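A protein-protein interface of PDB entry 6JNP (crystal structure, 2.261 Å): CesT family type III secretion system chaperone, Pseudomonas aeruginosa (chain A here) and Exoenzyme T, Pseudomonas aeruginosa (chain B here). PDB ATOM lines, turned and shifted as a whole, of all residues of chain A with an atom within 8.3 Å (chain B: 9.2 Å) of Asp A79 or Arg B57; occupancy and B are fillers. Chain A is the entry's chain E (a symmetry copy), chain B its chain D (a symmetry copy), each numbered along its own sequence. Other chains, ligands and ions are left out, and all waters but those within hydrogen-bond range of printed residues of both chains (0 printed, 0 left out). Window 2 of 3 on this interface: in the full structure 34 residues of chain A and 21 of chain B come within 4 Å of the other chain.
No residue of chain B comes within 4 Å of Arg A78.
Asp A79 touches just these residues of chain B: Trp B49 (3.8 Å), Leu B53 (3.8 Å) and Arg B57 (3.2 Å).
No residue of chain B comes within 4 Å of Pro A80.
Glu A81 touches none of the printed residues of chain B.
Ser A82 touches just one residue of chain B: Trp B49 (3.0 Å).
No residue of chain B comes within 4 Å of Gly A83.
Arg A85 touches none of the printed residues of chain B.
Of the printed residues of chain B, Leu A86 touches Trp B49 (3.5 Å) and Leu B53 (3.5 Å).
Of the printed residues of chain A, Trp B49 touches Asp A79 (3.8 Å), Ser A82 (3.0 Å), Glu A84 (3.7 Å) and Leu A86 (3.5 Å).
Printed residues of chain A within 4 Å of Leu B53: Asp A79 (3.8 Å) and Leu A86 (3.5 Å).
Ser B56 touches none of the printed residues of chain A.
Printed residues of chain A within 4 Å of Arg B57: His A42 (3.4 Å) and Asp A79 (3.2 Å).
The nearest residue of chain B that does not touch Asp A79 is Ser B56 (6.1 Å).
The nearest printed residue of chain A that does not touch Trp B49 is Glu A81 (5.8 Å).
O of Leu B54 lies close to NE2 of His A42, at 3.3 Å.
OG of Ser A82 lies within hydrogen-bond range of NE1 of Trp B49 (3.0 Å).
A ring nitrogen (NE2) of His A42 lies close to the backbone carbonyl oxygen of Arg B57 (3.5 Å).
Leu A48 touches Leu B54.
OD2 of Asp A79 touches NE1 of Trp B49 (3.8 Å).
CG of Asp A79 touches CD1 of Leu B53, at 3.8 Å.
CD of Arg B57 touches OD1 of Asp A79, 3.2 Å away.
Trp B49 touches Glu A84.
CD2 of Leu A86 touches CH2 of Trp B49, 3.5 Å away.
Leu B53 touches Leu A86 (CD2 to CD1, 3.5 Å).
Of the 16 printed residues of chain A, 6 touch a printed residue of chain B.
Among the printed residues, no Asp or Glu carboxylate lies within 4 Å of a Lys or Arg side-chain nitrogen of the other chain.
The backbone carbonyl oxygen (O) of Gly A77 sits at hydrogen-bond distance from the backbone NH (N) of Leu A86, 2.9 Å away.
O of His A42 is in hydrogen-bond range of NH1 of Arg A90 (2.8 Å).
The backbone carbonyl oxygen of Glu A84 sits at hydrogen-bond distance from the backbone NH of Asp A79 (2.9 Å).
OD1 of Asp A79 is in hydrogen-bond range of N of Glu A81, at 3.0 Å.
OD2 of Asp A79 lies within hydrogen-bond range of OG of Ser A82 (2.5 Å).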
ATOM      1  N   HIS A  42     -38.447  23.402   9.300  1.00  0.00           N
ATOM      2  CA  HIS A  42     -37.030  23.619   9.051  1.00  0.00           C
ATOM      3  C   HIS A  42     -36.840  24.372   7.739  1.00  0.00           C
ATOM      4  O   HIS A  42     -37.004  23.786   6.663  1.00  0.00           O
ATOM      5  CB  HIS A  42     -36.294  22.277   9.016  1.00  0.00           C
ATOM      6  CG  HIS A  42     -34.805  22.403   8.995  1.00  0.00           C
ATOM      7  ND1 HIS A  42     -34.107  22.828   7.884  1.00  0.00           N
ATOM      8  CD2 HIS A  42     -33.875  22.149   9.947  1.00  0.00           C
ATOM      9  CE1 HIS A  42     -32.814  22.837   8.155  1.00  0.00           C
ATOM     10  NE2 HIS A  42     -32.646  22.430   9.400  1.00  0.00           N
ATOM     11  N   PRO A  43     -36.517  25.672   7.778  1.00  0.00           N
ATOM     12  CA  PRO A  43     -36.411  26.461   9.009  1.00  0.00           C
ATOM     13  C   PRO A  43     -37.781  26.890   9.525  1.00  0.00           C
ATOM     14  O   PRO A  43     -38.795  26.318   9.117  1.00  0.00           O
ATOM     15  CB  PRO A  43     -35.590  27.671   8.570  1.00  0.00           C
ATOM     16  CG  PRO A  43     -35.984  27.862   7.143  1.00  0.00           C
ATOM     17  CD  PRO A  43     -36.193  26.474   6.585  1.00  0.00           C
ATOM     18  N   LEU A  48     -40.456  20.964   5.871  1.00  0.00           N
ATOM     19  CA  LEU A  48     -39.506  20.134   5.148  1.00  0.00           C
ATOM     20  C   LEU A  48     -39.923  18.676   5.282  1.00  0.00           C
ATOM     21  O   LEU A  48     -40.117  18.183   6.398  1.00  0.00           O
ATOM     22  CB  LEU A  48     -38.093  20.336   5.701  1.00  0.00           C
ATOM     23  CG  LEU A  48     -36.981  19.391   5.246  1.00  0.00           C
ATOM     24  CD1 LEU A  48     -36.470  19.792   3.878  1.00  0.00           C
ATOM     25  CD2 LEU A  48     -35.850  19.375   6.262  1.00  0.00           C
ATOM     26  N   ALA A  59     -26.594  10.187  -6.603  1.00  0.00           N
ATOM     27  CA  ALA A  59     -26.946  11.420  -5.915  1.00  0.00           C
ATOM     28  C   ALA A  59     -25.970  12.553  -6.195  1.00  0.00           C
ATOM     29  O   ALA A  59     -26.264  13.704  -5.857  1.00  0.00           O
ATOM     30  CB  ALA A  59     -27.028  11.179  -4.403  1.00  0.00           C
ATOM     31  N   LEU A  76     -32.376  15.461  -4.411  1.00  0.00           N
ATOM     32  CA  LEU A  76     -31.633  14.289  -3.961  1.00  0.00           C
ATOM     33  C   LEU A  76     -30.258  14.761  -3.500  1.00  0.00           C
ATOM     34  O   LEU A  76     -29.385  15.065  -4.318  1.00  0.00           O
ATOM     35  CB  LEU A  76     -31.527  13.250  -5.073  1.00  0.00           C
ATOM     36  CG  LEU A  76     -30.662  12.026  -4.763  1.00  0.00           C
ATOM     37  CD1 LEU A  76     -31.077  11.399  -3.445  1.00  0.00           C
ATOM     38  CD2 LEU A  76     -30.747  11.007  -5.886  1.00  0.00           C
ATOM     39  N   GLY A  77     -30.071  14.826  -2.182  1.00  0.00           N
ATOM     40  CA  GLY A  77     -28.813  15.216  -1.592  1.00  0.00           C
ATOM     41  C   GLY A  77     -28.221  14.097  -0.753  1.00  0.00           C
ATOM     42  O   GLY A  77     -28.752  12.987  -0.685  1.00  0.00           O
ATOM     43  N   ARG A  78     -27.107  14.418  -0.102  1.00  0.00           N
ATOM     44  CA  ARG A  78     -26.418  13.462   0.753  1.00  0.00           C
ATOM     45  C   ARG A  78     -25.872  14.187   1.970  1.00  0.00           C
ATOM     46  O   ARG A  78     -25.250  15.245   1.840  1.00  0.00           O
ATOM     47  CB  ARG A  78     -25.283  12.762  -0.001  1.00  0.00           C
ATOM     48  CG  ARG A  78     -24.495  11.756   0.827  1.00  0.00           C
ATOM     49  CD  ARG A  78     -23.486  11.017  -0.038  1.00  0.00           C
ATOM     50  NE  ARG A  78     -22.700  10.054   0.727  1.00  0.00           N
ATOM     51  CZ  ARG A  78     -21.529  10.328   1.292  1.00  0.00           C
ATOM     52  NH1 ARG A  78     -21.004  11.542   1.179  1.00  0.00           N
ATOM     53  NH2 ARG A  78     -20.881   9.391   1.968  1.00  0.00           N
ATOM     54  N   ASP A  79     -26.113  13.623   3.141  1.00  0.00           N
ATOM     55  CA  ASP A  79     -25.542  14.150   4.370  1.00  0.00           C
ATOM     56  C   ASP A  79     -24.064  13.785   4.430  1.00  0.00           C
ATOM     57  O   ASP A  79     -23.744  12.595   4.537  1.00  0.00           O
ATOM     58  CB  ASP A  79     -26.284  13.586   5.580  1.00  0.00           C
ATOM     59  CG  ASP A  79     -25.680  14.030   6.896  1.00  0.00           C
ATOM     60  OD1 ASP A  79     -24.996  15.073   6.917  1.00  0.00           O
ATOM     61  OD2 ASP A  79     -25.886  13.333   7.911  1.00  0.00           O
ATOM     62  N   PRO A  80     -23.140  14.748   4.365  1.00  0.00           N
ATOM     63  CA  PRO A  80     -21.717  14.390   4.467  1.00  0.00           C
ATOM     64  C   PRO A  80     -21.327  13.879   5.842  1.00  0.00           C
ATOM     65  O   PRO A  80     -20.307  13.187   5.960  1.00  0.00           O
ATOM     66  CB  PRO A  80     -20.998  15.702   4.128  1.00  0.00           C
ATOM     67  CG  PRO A  80     -21.964  16.759   4.520  1.00  0.00           C
ATOM     68  CD  PRO A  80     -23.332  16.200   4.223  1.00  0.00           C
ATOM     69  N   GLU A  81     -22.113  14.177   6.879  1.00  0.00           N
ATOM     70  CA  GLU A  81     -21.790  13.698   8.218  1.00  0.00           C
ATOM     71  C   GLU A  81     -22.004  12.193   8.326  1.00  0.00           C
ATOM     72  O   GLU A  81     -21.118  11.460   8.780  1.00  0.00           O
ATOM     73  CB  GLU A  81     -22.635  14.445   9.253  1.00  0.00           C
ATOM     74  CG  GLU A  81     -22.002  14.574  10.637  1.00  0.00           C
ATOM     75  CD  GLU A  81     -21.886  13.249  11.367  1.00  0.00           C
ATOM     76  OE1 GLU A  81     -20.801  12.634  11.319  1.00  0.00           O
ATOM     77  OE2 GLU A  81     -22.885  12.821  11.984  1.00  0.00           O
ATOM     78  N   SER A  82     -23.174  11.712   7.905  1.00  0.00           N
ATOM     79  CA  SER A  82     -23.521  10.304   8.042  1.00  0.00           C
ATOM     80  C   SER A  82     -23.362   9.506   6.755  1.00  0.00           C
ATOM     81  O   SER A  82     -23.338   8.271   6.813  1.00  0.00           O
ATOM     82  CB  SER A  82     -24.966  10.166   8.536  1.00  0.00           C
ATOM     83  OG  SER A  82     -25.862  10.847   7.675  1.00  0.00           O
ATOM     84  N   GLY A  83     -23.253  10.169   5.607  1.00  0.00           N
ATOM     85  CA  GLY A  83     -23.192   9.475   4.336  1.00  0.00           C
ATOM     86  C   GLY A  83     -24.523   9.006   3.798  1.00  0.00           C
ATOM     87  O   GLY A  83     -24.548   8.288   2.791  1.00  0.00           O
ATOM     88  N   GLU A  84     -25.628   9.393   4.430  1.00  0.00           N
ATOM     89  CA  GLU A  84     -26.948   8.928   4.027  1.00  0.00           C
ATOM     90  C   GLU A  84     -27.497   9.788   2.897  1.00  0.00           C
ATOM     91  O   GLU A  84     -27.414  11.019   2.943  1.00  0.00           O
ATOM     92  CB  GLU A  84     -27.902   8.954   5.219  1.00  0.00           C
ATOM     93  CG  GLU A  84     -27.485   8.044   6.366  1.00  0.00           C
ATOM     94  CD  GLU A  84     -28.080   6.656   6.253  1.00  0.00           C
ATOM     95  OE1 GLU A  84     -28.641   6.171   7.255  1.00  0.00           O
ATOM     96  OE2 GLU A  84     -27.997   6.054   5.162  1.00  0.00           O
ATOM     97  N   ARG A  85     -28.056   9.136   1.881  1.00  0.00           N
ATOM     98  CA  ARG A  85     -28.705   9.843   0.785  1.00  0.00           C
ATOM     99  C   ARG A  85     -30.141  10.178   1.167  1.00  0.00           C
ATOM    100  O   ARG A  85     -30.872   9.325   1.681  1.00  0.00           O
ATOM    101  CB  ARG A  85     -28.666   9.002  -0.490  1.00  0.00           C
ATOM    102  CG  ARG A  85     -27.307   9.000  -1.164  1.00  0.00           C
ATOM    103  CD  ARG A  85     -27.184   7.913  -2.219  1.00  0.00           C
ATOM    104  NE  ARG A  85     -28.088   8.096  -3.351  1.00  0.00           N
ATOM    105  CZ  ARG A  85     -28.998   7.206  -3.730  1.00  0.00           C
ATOM    106  NH1 ARG A  85     -29.123   6.062  -3.072  1.00  0.00           N
ATOM    107  NH2 ARG A  85     -29.775   7.452  -4.775  1.00  0.00           N
ATOM    108  N   LEU A  86     -30.540  11.422   0.920  1.00  0.00           N
ATOM    109  CA  LEU A  86     -31.836  11.935   1.330  1.00  0.00           C
ATOM    110  C   LEU A  86     -32.560  12.548   0.142  1.00  0.00           C
ATOM    111  O   LEU A  86     -31.943  13.109  -0.767  1.00  0.00           O
ATOM    112  CB  LEU A  86     -31.697  12.985   2.436  1.00  0.00           C
ATOM    113  CG  LEU A  86     -30.975  12.507   3.695  1.00  0.00           C
ATOM    114  CD1 LEU A  86     -30.789  13.656   4.660  1.00  0.00           C
ATOM    115  CD2 LEU A  86     -31.751  11.376   4.346  1.00  0.00           C
ATOM    116  N   ARG A  90     -39.550  21.122   0.327  1.00  0.00           N
ATOM    117  CA  ARG A  90     -39.839  22.116   1.350  1.00  0.00           C
ATOM    118  C   ARG A  90     -40.826  23.141   0.813  1.00  0.00           C
ATOM    119  O   ARG A  90     -40.719  23.571  -0.339  1.00  0.00           O
ATOM    120  CB  ARG A  90     -38.555  22.812   1.819  1.00  0.00           C
ATOM    121  CG  ARG A  90     -38.781  23.961   2.783  1.00  0.00           C
ATOM    122  CD  ARG A  90     -37.573  24.166   3.676  1.00  0.00           C
ATOM    123  NE  ARG A  90     -36.354  24.440   2.922  1.00  0.00           N
ATOM    124  CZ  ARG A  90     -35.129  24.346   3.430  1.00  0.00           C
ATOM    125  NH1 ARG A  90     -34.958  23.974   4.692  1.00  0.00           N
ATOM    126  NH2 ARG A  90     -34.074  24.617   2.675  1.00  0.00           N
ATOM    127  N   TRP B  49     -30.694  10.492  15.006  1.00  0.00           N
ATOM    128  CA  TRP B  49     -30.031  10.937  13.786  1.00  0.00           C
ATOM    129  C   TRP B  49     -30.800  12.075  13.127  1.00  0.00           C
ATOM    130  O   TRP B  49     -30.198  13.027  12.616  1.00  0.00           O
ATOM    131  CB  TRP B  49     -29.865   9.759  12.826  1.00  0.00           C
ATOM    132  CG  TRP B  49     -29.351  10.145  11.477  1.00  0.00           C
ATOM    133  CD1 TRP B  49     -28.063  10.454  11.148  1.00  0.00           C
ATOM    134  CD2 TRP B  49     -30.113  10.256  10.270  1.00  0.00           C
ATOM    135  NE1 TRP B  49     -27.978  10.754   9.810  1.00  0.00           N
ATOM    136  CE2 TRP B  49     -29.223  10.640   9.249  1.00  0.00           C
ATOM    137  CE3 TRP B  49     -31.462  10.070   9.954  1.00  0.00           C
ATOM    138  CZ2 TRP B  49     -29.637  10.841   7.934  1.00  0.00           C
ATOM    139  CZ3 TRP B  49     -31.871  10.270   8.649  1.00  0.00           C
ATOM    140  CH2 TRP B  49     -30.963  10.652   7.656  1.00  0.00           C
ATOM    141  N   LEU B  50     -32.134  12.001  13.138  1.00  0.00           N
ATOM    142  CA  LEU B  50     -32.947  13.090  12.607  1.00  0.00           C
ATOM    143  C   LEU B  50     -32.738  14.370  13.403  1.00  0.00           C
ATOM    144  O   LEU B  50     -32.668  15.461  12.829  1.00  0.00           O
ATOM    145  CB  LEU B  50     -34.425  12.704  12.613  1.00  0.00           C
ATOM    146  CG  LEU B  50     -34.874  11.615  11.642  1.00  0.00           C
ATOM    147  CD1 LEU B  50     -36.375  11.401  11.734  1.00  0.00           C
ATOM    148  CD2 LEU B  50     -34.467  11.971  10.231  1.00  0.00           C
ATOM    149  N   GLY B  51     -32.661  14.256  14.730  1.00  0.00           N
ATOM    150  CA  GLY B  51     -32.402  15.432  15.546  1.00  0.00           C
ATOM    151  C   GLY B  51     -31.061  16.064  15.229  1.00  0.00           C
ATOM    152  O   GLY B  51     -30.954  17.285  15.072  1.00  0.00           O
ATOM    153  N   LYS B  52     -30.018  15.236  15.122  1.00  0.00           N
ATOM    154  CA  LYS B  52     -28.699  15.746  14.755  1.00  0.00           C
ATOM    155  C   LYS B  52     -28.723  16.403  13.380  1.00  0.00           C
ATOM    156  O   LYS B  52     -28.102  17.453  13.173  1.00  0.00           O
ATOM    157  CB  LYS B  52     -27.668  14.616  14.777  1.00  0.00           C
ATOM    158  CG  LYS B  52     -27.558  13.876  16.098  1.00  0.00           C
ATOM    159  CD  LYS B  52     -26.780  12.579  15.925  1.00  0.00           C
ATOM    160  CE  LYS B  52     -26.917  11.678  17.143  1.00  0.00           C
ATOM    161  NZ  LYS B  52     -26.282  10.348  16.923  1.00  0.00           N
ATOM    162  N   LEU B  53     -29.440  15.801  12.430  1.00  0.00           N
ATOM    163  CA  LEU B  53     -29.463  16.315  11.065  1.00  0.00           C
ATOM    164  C   LEU B  53     -30.218  17.635  10.975  1.00  0.00           C
ATOM    165  O   LEU B  53     -29.781  18.562  10.283  1.00  0.00           O
ATOM    166  CB  LEU B  53     -30.088  15.275  10.137  1.00  0.00           C
ATOM    167  CG  LEU B  53     -30.263  15.652   8.669  1.00  0.00           C
ATOM    168  CD1 LEU B  53     -28.925  15.639   7.946  1.00  0.00           C
ATOM    169  CD2 LEU B  53     -31.255  14.711   8.012  1.00  0.00           C
ATOM    170  N   LEU B  54     -31.357  17.738  11.661  1.00  0.00           N
ATOM    171  CA  LEU B  54     -32.154  18.956  11.622  1.00  0.00           C
ATOM    172  C   LEU B  54     -31.600  20.048  12.525  1.00  0.00           C
ATOM    173  O   LEU B  54     -31.989  21.211  12.377  1.00  0.00           O
ATOM    174  CB  LEU B  54     -33.601  18.648  12.009  1.00  0.00           C
ATOM    175  CG  LEU B  54     -34.324  17.657  11.092  1.00  0.00           C
ATOM    176  CD1 LEU B  54     -35.667  17.261  11.679  1.00  0.00           C
ATOM    177  CD2 LEU B  54     -34.494  18.237   9.695  1.00  0.00           C
ATOM    178  N   GLY B  55     -30.709  19.706  13.454  1.00  0.00           N
ATOM    179  CA  GLY B  55     -30.072  20.711  14.280  1.00  0.00           C
ATOM    180  C   GLY B  55     -28.788  21.242  13.678  1.00  0.00           C
ATOM    181  O   GLY B  55     -28.462  22.423  13.836  1.00  0.00           O
ATOM    182  N   SER B  56     -28.051  20.379  12.980  1.00  0.00           N
ATOM    183  CA  SER B  56     -26.770  20.750  12.394  1.00  0.00           C
ATOM    184  C   SER B  56     -26.863  21.134  10.924  1.00  0.00           C
ATOM    185  O   SER B  56     -26.123  22.018  10.480  1.00  0.00           O
ATOM    186  CB  SER B  56     -25.765  19.603  12.544  1.00  0.00           C
ATOM    187  OG  SER B  56     -26.219  18.436  11.879  1.00  0.00           O
ATOM    188  N   ARG B  57     -27.746  20.499  10.161  1.00  0.00           N
ATOM    189  CA  ARG B  57     -27.854  20.780   8.733  1.00  0.00           C
ATOM    190  C   ARG B  57     -29.242  21.299   8.375  1.00  0.00           C
ATOM    191  O   ARG B  57     -29.421  22.486   8.105  1.00  0.00           O
ATOM    192  CB  ARG B  57     -27.534  19.525   7.917  1.00  0.00           C
ATOM    193  CG  ARG B  57     -26.621  18.538   8.629  1.00  0.00           C
ATOM    194  CD  ARG B  57     -25.441  18.123   7.762  1.00  0.00           C
ATOM    195  NE  ARG B  57     -24.420  19.165   7.672  1.00  0.00           N
ATOM    196  CZ  ARG B  57     -24.296  20.009   6.653  1.00  0.00           C
ATOM    197  NH1 ARG B  57     -23.333  20.922   6.663  1.00  0.00           N
ATOM    198  NH2 ARG B  57     -25.127  19.941   5.624  1.00  0.00           N
